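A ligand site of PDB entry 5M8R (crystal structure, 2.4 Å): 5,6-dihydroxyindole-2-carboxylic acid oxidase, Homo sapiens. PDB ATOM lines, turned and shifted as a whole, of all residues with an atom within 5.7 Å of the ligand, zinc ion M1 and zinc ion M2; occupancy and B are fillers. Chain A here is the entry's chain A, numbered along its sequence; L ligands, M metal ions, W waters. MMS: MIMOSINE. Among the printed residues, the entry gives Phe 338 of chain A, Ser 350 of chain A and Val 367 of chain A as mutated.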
ATOM      1  N   HIS A 168      -1.508   4.963   5.050  1.00  0.00           N
ATOM      2  CA  HIS A 168      -0.783   4.430   3.905  1.00  0.00           C
ATOM      3  C   HIS A 168       0.329   3.483   4.350  1.00  0.00           C
ATOM      4  O   HIS A 168       0.530   2.423   3.735  1.00  0.00           O
ATOM      5  CB  HIS A 168      -0.209   5.599   3.076  1.00  0.00           C
ATOM      6  CG  HIS A 168       0.247   5.227   1.693  1.00  0.00           C
ATOM      7  ND1 HIS A 168       1.570   5.006   1.374  1.00  0.00           N
ATOM      8  CD2 HIS A 168      -0.435   5.105   0.527  1.00  0.00           C
ATOM      9  CE1 HIS A 168       1.675   4.719   0.085  1.00  0.00           C
ATOM     10  NE2 HIS A 168       0.475   4.781  -0.456  1.00  0.00           N
ATOM     11  N   SER A 190      -2.912  -1.885  -0.556  1.00  0.00           N
ATOM     12  CA  SER A 190      -3.293  -0.702  -1.309  1.00  0.00           C
ATOM     13  C   SER A 190      -2.562  -0.522  -2.636  1.00  0.00           C
ATOM     14  O   SER A 190      -2.841   0.452  -3.333  1.00  0.00           O
ATOM     15  CB  SER A 190      -3.064   0.552  -0.466  1.00  0.00           C
ATOM     16  OG  SER A 190      -1.711   0.591  -0.032  1.00  0.00           O
ATOM     17  N   HIS A 191      -1.661  -1.440  -3.003  1.00  0.00           N
ATOM     18  CA  HIS A 191      -0.935  -1.370  -4.263  1.00  0.00           C
ATOM     19  C   HIS A 191      -0.843  -2.756  -4.855  1.00  0.00           C
ATOM     20  O   HIS A 191      -1.137  -3.753  -4.196  1.00  0.00           O
ATOM     21  CB  HIS A 191       0.483  -0.802  -4.087  1.00  0.00           C
ATOM     22  CG  HIS A 191       0.513   0.458  -3.307  1.00  0.00           C
ATOM     23  ND1 HIS A 191       0.320   0.507  -1.941  1.00  0.00           N
ATOM     24  CD2 HIS A 191       0.658   1.744  -3.711  1.00  0.00           C
ATOM     25  CE1 HIS A 191       0.368   1.758  -1.540  1.00  0.00           C
ATOM     26  NE2 HIS A 191       0.581   2.530  -2.583  1.00  0.00           N
ATOM     27  N   PHE A 196      -6.005  -0.574  -5.718  1.00  0.00           N
ATOM     28  CA  PHE A 196      -5.062   0.543  -5.720  1.00  0.00           C
ATOM     29  C   PHE A 196      -5.784   1.884  -5.902  1.00  0.00           C
ATOM     30  O   PHE A 196      -5.542   2.842  -5.158  1.00  0.00           O
ATOM     31  CB  PHE A 196      -4.014   0.342  -6.823  1.00  0.00           C
ATOM     32  CG  PHE A 196      -3.264   1.608  -7.183  1.00  0.00           C
ATOM     33  CD1 PHE A 196      -2.274   2.113  -6.354  1.00  0.00           C
ATOM     34  CD2 PHE A 196      -3.566   2.298  -8.357  1.00  0.00           C
ATOM     35  CE1 PHE A 196      -1.606   3.293  -6.680  1.00  0.00           C
ATOM     36  CE2 PHE A 196      -2.900   3.464  -8.680  1.00  0.00           C
ATOM     37  CZ  PHE A 196      -1.918   3.962  -7.853  1.00  0.00           C
ATOM     38  N   TRP A 199      -8.660   2.454  -3.122  1.00  0.00           N
ATOM     39  CA  TRP A 199      -7.999   2.750  -1.847  1.00  0.00           C
ATOM     40  C   TRP A 199      -7.529   4.201  -1.810  1.00  0.00           C
ATOM     41  O   TRP A 199      -7.869   4.954  -0.891  1.00  0.00           O
ATOM     42  CB  TRP A 199      -6.808   1.796  -1.603  1.00  0.00           C
ATOM     43  CG  TRP A 199      -6.262   1.852  -0.182  1.00  0.00           C
ATOM     44  CD1 TRP A 199      -6.506   0.952   0.816  1.00  0.00           C
ATOM     45  CD2 TRP A 199      -5.415   2.870   0.387  1.00  0.00           C
ATOM     46  NE1 TRP A 199      -5.873   1.348   1.979  1.00  0.00           N
ATOM     47  CE2 TRP A 199      -5.193   2.505   1.734  1.00  0.00           C
ATOM     48  CE3 TRP A 199      -4.835   4.048  -0.108  1.00  0.00           C
ATOM     49  CZ2 TRP A 199      -4.388   3.293   2.607  1.00  0.00           C
ATOM     50  CZ3 TRP A 199      -4.029   4.819   0.759  1.00  0.00           C
ATOM     51  CH2 TRP A 199      -3.822   4.442   2.102  1.00  0.00           C
ATOM     52  N   HIS A 200      -6.724   4.611  -2.802  1.00  0.00           N
ATOM     53  CA  HIS A 200      -6.139   5.957  -2.794  1.00  0.00           C
ATOM     54  C   HIS A 200      -7.199   7.023  -2.974  1.00  0.00           C
ATOM     55  O   HIS A 200      -7.011   8.142  -2.500  1.00  0.00           O
ATOM     56  CB  HIS A 200      -5.046   6.079  -3.859  1.00  0.00           C
ATOM     57  CG  HIS A 200      -3.766   5.395  -3.470  1.00  0.00           C
ATOM     58  ND1 HIS A 200      -3.589   4.034  -3.568  1.00  0.00           N
ATOM     59  CD2 HIS A 200      -2.620   5.884  -2.918  1.00  0.00           C
ATOM     60  CE1 HIS A 200      -2.391   3.710  -3.121  1.00  0.00           C
ATOM     61  NE2 HIS A 200      -1.776   4.812  -2.736  1.00  0.00           N
ATOM     62  N   ARG A 297      19.476   5.522 -12.894  1.00  0.00           N
ATOM     63  CA  ARG A 297      18.300   4.933 -13.534  1.00  0.00           C
ATOM     64  C   ARG A 297      17.645   5.943 -14.469  1.00  0.00           C
ATOM     65  O   ARG A 297      16.597   6.525 -14.162  1.00  0.00           O
ATOM     66  CB  ARG A 297      17.319   4.447 -12.477  1.00  0.00           C
ATOM     67  CG  ARG A 297      16.280   3.508 -13.001  1.00  0.00           C
ATOM     68  CD  ARG A 297      15.627   2.812 -11.848  1.00  0.00           C
ATOM     69  NE  ARG A 297      14.398   2.153 -12.239  1.00  0.00           N
ATOM     70  CZ  ARG A 297      13.468   1.772 -11.373  1.00  0.00           C
ATOM     71  NH1 ARG A 297      13.658   2.014 -10.078  1.00  0.00           N
ATOM     72  NH2 ARG A 297      12.363   1.176 -11.793  1.00  0.00           N
ATOM     73  N   GLU A 336      -1.551   2.625 -12.644  1.00  0.00           N
ATOM     74  CA  GLU A 336      -0.682   2.455 -11.494  1.00  0.00           C
ATOM     75  C   GLU A 336       0.777   2.517 -11.915  1.00  0.00           C
ATOM     76  O   GLU A 336       1.606   3.096 -11.209  1.00  0.00           O
ATOM     77  CB  GLU A 336      -0.978   1.145 -10.752  1.00  0.00           C
ATOM     78  CG  GLU A 336      -0.088   1.034  -9.506  1.00  0.00           C
ATOM     79  CD  GLU A 336      -0.390  -0.139  -8.603  1.00  0.00           C
ATOM     80  OE1 GLU A 336      -1.308  -0.919  -8.910  1.00  0.00           O
ATOM     81  OE2 GLU A 336       0.309  -0.260  -7.561  1.00  0.00           O
ATOM     82  N   PHE A 338       2.813  -0.256 -13.644  1.00  0.00           N
ATOM     83  CA  PHE A 338       3.632  -1.445 -13.841  1.00  0.00           C
ATOM     84  C   PHE A 338       3.610  -1.971 -15.269  1.00  0.00           C
ATOM     85  O   PHE A 338       4.482  -2.752 -15.646  1.00  0.00           O
ATOM     86  CB  PHE A 338       3.187  -2.565 -12.896  1.00  0.00           C
ATOM     87  CG  PHE A 338       3.516  -2.293 -11.462  1.00  0.00           C
ATOM     88  CD1 PHE A 338       4.823  -2.416 -11.001  1.00  0.00           C
ATOM     89  CD2 PHE A 338       2.515  -1.890 -10.582  1.00  0.00           C
ATOM     90  CE1 PHE A 338       5.144  -2.154  -9.660  1.00  0.00           C
ATOM     91  CE2 PHE A 338       2.823  -1.627  -9.247  1.00  0.00           C
ATOM     92  CZ  PHE A 338       4.144  -1.767  -8.786  1.00  0.00           C
ATOM     93  N   SER A 350       8.651   1.465 -15.605  1.00  0.00           N
ATOM     94  CA  SER A 350       7.834   2.227 -14.688  1.00  0.00           C
ATOM     95  C   SER A 350       7.275   3.386 -15.485  1.00  0.00           C
ATOM     96  O   SER A 350       8.019   4.066 -16.198  1.00  0.00           O
ATOM     97  CB  SER A 350       8.627   2.719 -13.478  1.00  0.00           C
ATOM     98  OG  SER A 350       9.846   3.292 -13.906  1.00  0.00           O
ATOM     99  N   HIS A 353       1.777   6.664 -12.804  1.00  0.00           N
ATOM    100  CA  HIS A 353       1.809   6.963 -11.360  1.00  0.00           C
ATOM    101  C   HIS A 353       3.096   6.481 -10.697  1.00  0.00           C
ATOM    102  O   HIS A 353       3.677   7.187  -9.872  1.00  0.00           O
ATOM    103  CB  HIS A 353       0.578   6.347 -10.683  1.00  0.00           C
ATOM    104  CG  HIS A 353       0.796   5.964  -9.252  1.00  0.00           C
ATOM    105  ND1 HIS A 353       1.217   4.711  -8.873  1.00  0.00           N
ATOM    106  CD2 HIS A 353       0.656   6.678  -8.110  1.00  0.00           C
ATOM    107  CE1 HIS A 353       1.328   4.657  -7.560  1.00  0.00           C
ATOM    108  NE2 HIS A 353       0.986   5.846  -7.063  1.00  0.00           N
ATOM    109  N   ASN A 354       3.550   5.266 -11.027  1.00  0.00           N
ATOM    110  CA  ASN A 354       4.817   4.793 -10.479  1.00  0.00           C
ATOM    111  C   ASN A 354       5.972   5.705 -10.904  1.00  0.00           C
ATOM    112  O   ASN A 354       6.838   6.042 -10.083  1.00  0.00           O
ATOM    113  CB  ASN A 354       5.085   3.357 -10.925  1.00  0.00           C
ATOM    114  CG  ASN A 354       4.266   2.335 -10.166  1.00  0.00           C
ATOM    115  OD1 ASN A 354       3.757   2.598  -9.075  1.00  0.00           O
ATOM    116  ND2 ASN A 354       4.169   1.138 -10.710  1.00  0.00           N
ATOM    117  N   HIS A 357       6.346   8.879  -9.034  1.00  0.00           N
ATOM    118  CA  HIS A 357       6.932   8.655  -7.716  1.00  0.00           C
ATOM    119  C   HIS A 357       8.440   8.555  -7.799  1.00  0.00           C
ATOM    120  O   HIS A 357       9.164   9.173  -7.005  1.00  0.00           O
ATOM    121  CB  HIS A 357       6.397   7.368  -7.097  1.00  0.00           C
ATOM    122  CG  HIS A 357       5.131   7.516  -6.324  1.00  0.00           C
ATOM    123  ND1 HIS A 357       5.088   8.053  -5.047  1.00  0.00           N
ATOM    124  CD2 HIS A 357       3.854   7.160  -6.612  1.00  0.00           C
ATOM    125  CE1 HIS A 357       3.844   8.026  -4.602  1.00  0.00           C
ATOM    126  NE2 HIS A 357       3.085   7.490  -5.529  1.00  0.00           N
ATOM    127  N   LEU A 358       8.924   7.700  -8.709  1.00  0.00           N
ATOM    128  CA  LEU A 358      10.358   7.470  -8.857  1.00  0.00           C
ATOM    129  C   LEU A 358      11.078   8.726  -9.332  1.00  0.00           C
ATOM    130  O   LEU A 358      12.227   8.978  -8.924  1.00  0.00           O
ATOM    131  CB  LEU A 358      10.594   6.312  -9.840  1.00  0.00           C
ATOM    132  CG  LEU A 358       9.897   5.017  -9.389  1.00  0.00           C
ATOM    133  CD1 LEU A 358      10.056   3.934 -10.409  1.00  0.00           C
ATOM    134  CD2 LEU A 358      10.396   4.542  -8.013  1.00  0.00           C
ATOM    135  N   GLY A 364       9.392  10.685  -1.520  1.00  0.00           N
ATOM    136  CA  GLY A 364       8.212  10.378  -2.329  1.00  0.00           C
ATOM    137  C   GLY A 364       8.338   9.153  -3.218  1.00  0.00           C
ATOM    138  O   GLY A 364       7.325   8.718  -3.803  1.00  0.00           O
ATOM    139  N   GLY A 365       9.528   8.581  -3.333  1.00  0.00           N
ATOM    140  CA  GLY A 365       9.709   7.391  -4.137  1.00  0.00           C
ATOM    141  C   GLY A 365       9.670   6.097  -3.381  1.00  0.00           C
ATOM    142  O   GLY A 365       9.855   5.036  -3.980  1.00  0.00           O
ATOM    143  N   GLN A 366       9.453   6.126  -2.066  1.00  0.00           N
ATOM    144  CA  GLN A 366       9.439   4.928  -1.246  1.00  0.00           C
ATOM    145  C   GLN A 366       8.025   4.711  -0.710  1.00  0.00           C
ATOM    146  O   GLN A 366       7.485   5.594  -0.043  1.00  0.00           O
ATOM    147  CB  GLN A 366      10.425   5.050  -0.094  1.00  0.00           C
ATOM    148  CG  GLN A 366      11.806   5.410  -0.540  1.00  0.00           C
ATOM    149  CD  GLN A 366      12.729   5.598   0.653  1.00  0.00           C
ATOM    150  OE1 GLN A 366      13.107   6.721   0.976  1.00  0.00           O
ATOM    151  NE2 GLN A 366      13.051   4.509   1.337  1.00  0.00           N
ATOM    152  N   VAL A 367       7.460   3.532  -0.990  1.00  0.00           N
ATOM    153  CA  VAL A 367       6.009   3.343  -0.826  1.00  0.00           C
ATOM    154  C   VAL A 367       5.584   3.439   0.644  1.00  0.00           C
ATOM    155  O   VAL A 367       4.494   3.930   0.936  1.00  0.00           O
ATOM    156  CB  VAL A 367       5.573   2.020  -1.495  1.00  0.00           C
ATOM    157  CG1 VAL A 367       6.068   0.842  -0.747  1.00  0.00           C
ATOM    158  CG2 VAL A 367       4.046   1.955  -1.658  1.00  0.00           C
ATOM    159  N   SER A 370       6.044   7.588   1.152  1.00  0.00           N
ATOM    160  CA  SER A 370       5.881   8.623   0.147  1.00  0.00           C
ATOM    161  C   SER A 370       4.833   9.697   0.488  1.00  0.00           C
ATOM    162  O   SER A 370       5.056  10.840   0.073  1.00  0.00           O
ATOM    163  CB  SER A 370       5.619   7.949  -1.201  1.00  0.00           C
ATOM    164  OG  SER A 370       4.455   7.149  -1.172  1.00  0.00           O
ATOM    165  N   PHE A 376       2.695  13.997  -2.871  1.00  0.00           N
ATOM    166  CA  PHE A 376       1.869  12.801  -2.926  1.00  0.00           C
ATOM    167  C   PHE A 376       0.389  13.149  -3.147  1.00  0.00           C
ATOM    168  O   PHE A 376      -0.280  12.544  -3.998  1.00  0.00           O
ATOM    169  CB  PHE A 376       2.071  12.019  -1.622  1.00  0.00           C
ATOM    170  CG  PHE A 376       1.273  10.729  -1.532  1.00  0.00           C
ATOM    171  CD1 PHE A 376      -0.054  10.747  -1.164  1.00  0.00           C
ATOM    172  CD2 PHE A 376       1.881   9.512  -1.788  1.00  0.00           C
ATOM    173  CE1 PHE A 376      -0.786   9.580  -1.056  1.00  0.00           C
ATOM    174  CE2 PHE A 376       1.166   8.341  -1.683  1.00  0.00           C
ATOM    175  CZ  PHE A 376      -0.183   8.370  -1.317  1.00  0.00           C
ATOM    176  N   LEU A 379      -0.028  14.386  -6.743  1.00  0.00           N
ATOM    177  CA  LEU A 379       0.228  13.253  -7.620  1.00  0.00           C
ATOM    178  C   LEU A 379      -0.953  12.278  -7.638  1.00  0.00           C
ATOM    179  O   LEU A 379      -1.294  11.712  -8.689  1.00  0.00           O
ATOM    180  CB  LEU A 379       1.523  12.560  -7.153  1.00  0.00           C
ATOM    181  CG  LEU A 379       2.186  11.396  -7.882  1.00  0.00           C
ATOM    182  CD1 LEU A 379       3.555  11.174  -7.235  1.00  0.00           C
ATOM    183  CD2 LEU A 379       1.367  10.113  -7.781  1.00  0.00           C
ATOM    184  N   HIS A 380      -1.603  12.082  -6.487  1.00  0.00           N
ATOM    185  CA  HIS A 380      -2.739  11.157  -6.429  1.00  0.00           C
ATOM    186  C   HIS A 380      -4.090  11.782  -6.753  1.00  0.00           C
ATOM    187  O   HIS A 380      -4.957  11.076  -7.255  1.00  0.00           O
ATOM    188  CB  HIS A 380      -2.815  10.476  -5.060  1.00  0.00           C
ATOM    189  CG  HIS A 380      -2.119   9.154  -5.058  1.00  0.00           C
ATOM    190  ND1 HIS A 380      -2.643   8.038  -5.671  1.00  0.00           N
ATOM    191  CD2 HIS A 380      -0.886   8.806  -4.622  1.00  0.00           C
ATOM    192  CE1 HIS A 380      -1.780   7.053  -5.587  1.00  0.00           C
ATOM    193  NE2 HIS A 380      -0.713   7.482  -4.939  1.00  0.00           N
HETATM  194  O4  MMS L   1       2.751   3.822  -5.006  1.00  0.00           O
HETATM  195  C1  MMS L   1       7.629   0.768  -8.365  1.00  0.00           C
HETATM  196  O1  MMS L   1       7.695   1.340  -9.487  1.00  0.00           O
HETATM  197  O2  MMS L   1       8.331  -0.256  -8.129  1.00  0.00           O
HETATM  198  N1  MMS L   1       6.919   0.573  -6.023  1.00  0.00           N
HETATM  199  C2  MMS L   1       6.706   1.302  -7.269  1.00  0.00           C
HETATM  200  C3  MMS L   1       7.050   2.771  -7.092  1.00  0.00           C
HETATM  201  N2  MMS L   1       6.288   3.414  -6.056  1.00  0.00           N
HETATM  202  C8  MMS L   1       4.811   3.297  -6.029  1.00  0.00           C
HETATM  203  C4  MMS L   1       7.000   4.219  -5.014  1.00  0.00           C
HETATM  204  C7  MMS L   1       4.137   3.900  -5.065  1.00  0.00           C
HETATM  205  C5  MMS L   1       6.321   4.829  -4.054  1.00  0.00           C
HETATM  206  C6  MMS L   1       4.823   4.719  -4.017  1.00  0.00           C
HETATM  207  O3  MMS L   1       4.170   5.254  -3.183  1.00  0.00           O
HETATM  208 ZN    ZN M   1       1.228   6.585  -5.135  1.00  0.00          ZN
HETATM  209 ZN    ZN M   2       0.182   4.539  -2.422  1.00  0.00          ZN
HETATM  210  O   HOH W   1       2.278   1.194  -7.149  1.00  0.00           O
HETATM  211  O   HOH W   2       1.678   5.484  -3.522  1.00  0.00           O
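Water W1 lies within hydrogen-bond range of the side-chain carboxylate (OE2) of Glu 336 (2.5 Å), the side-chain amide oxygen (OD1) of Asn 354 (2.8 Å) and an oxygen (O4) of the ligand (3.4 Å).
Residues that only touch zinc ion M2: Phe 376.
Of the 22 residues printed, 5 come within 4 Å of zinc ion M2.
NE2 of His 200 binds zinc ion M2, 2.0 Å away.
NE2 of His 168 binds zinc ion M2 (2.0 Å).
NE2 of His 191 binds zinc ion M2.
Zinc ion M2 is bound by water W2, at 2.1 Å.
Zinc ion M2 has four donor atoms within binding distance.
Residues that only touch the ligand: Gly 365 (3.1 Å), Asn 354 (3.3 Å), Val 367 (3.5 Å), Leu 358 (3.6 Å) and Gln 366 (3.8 Å).
Hydrophobic or aromatic side chains within 4 Å of the ligand: His 191, His 353, His 357, Leu 358 and Val 367.
Zinc ion M1 is bound by water W2, NE2 of His 353, NE2 of His 357 and NE2 of His 380.
Zinc ion M1 has four donor atoms within binding distance.
ND1 of His 168 sits close to O of Val 367.
A ring nitrogen (ND1) of His 353 is in hydrogen-bond range of the backbone carbonyl oxygen (O) of Glu 336.
A ring nitrogen (ND1) of His 357 lies within hydrogen-bond range of the backbone carbonyl oxygen of Gly 364, at 2.6 Å.
A ring nitrogen (ND1) of His 353 sits at hydrogen-bond distance from the side-chain amide oxygen of Asn 354 (3.3 Å).
A ring nitrogen (ND1) of His 191 lies within hydrogen-bond range of the side-chain hydroxyl of Ser 190 (2.8 Å).
The backbone carbonyl oxygen of Phe 196 sits at hydrogen-bond distance from a ring nitrogen (ND1) of His 200 (2.8 Å).
N of Asn 354 lies within hydrogen-bond range of O of Glu 336.
Phe 376 touches zinc ion M1 (CE2 to ZN, 3.9 Å).
Of the 22 residues printed, 4 come within 4 Å of zinc ion M1.
Along chain A the residues within 4 Å of zinc ion M1 span positions 353 to 380.
The nearest printed residue that does not touch zinc ion M1 is His 200 (4.2 Å).
A ring nitrogen (NE2) of His 191 sits close to an oxygen (O4) of the ligand (3.5 Å).
OG of Ser 370 lies within hydrogen-bond range of O3 of the ligand.
ND1 of His 357 sits close to O3 of the ligand (3.5 Å).
NE2 of His 353 sits close to O4 of the ligand (3.4 Å).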
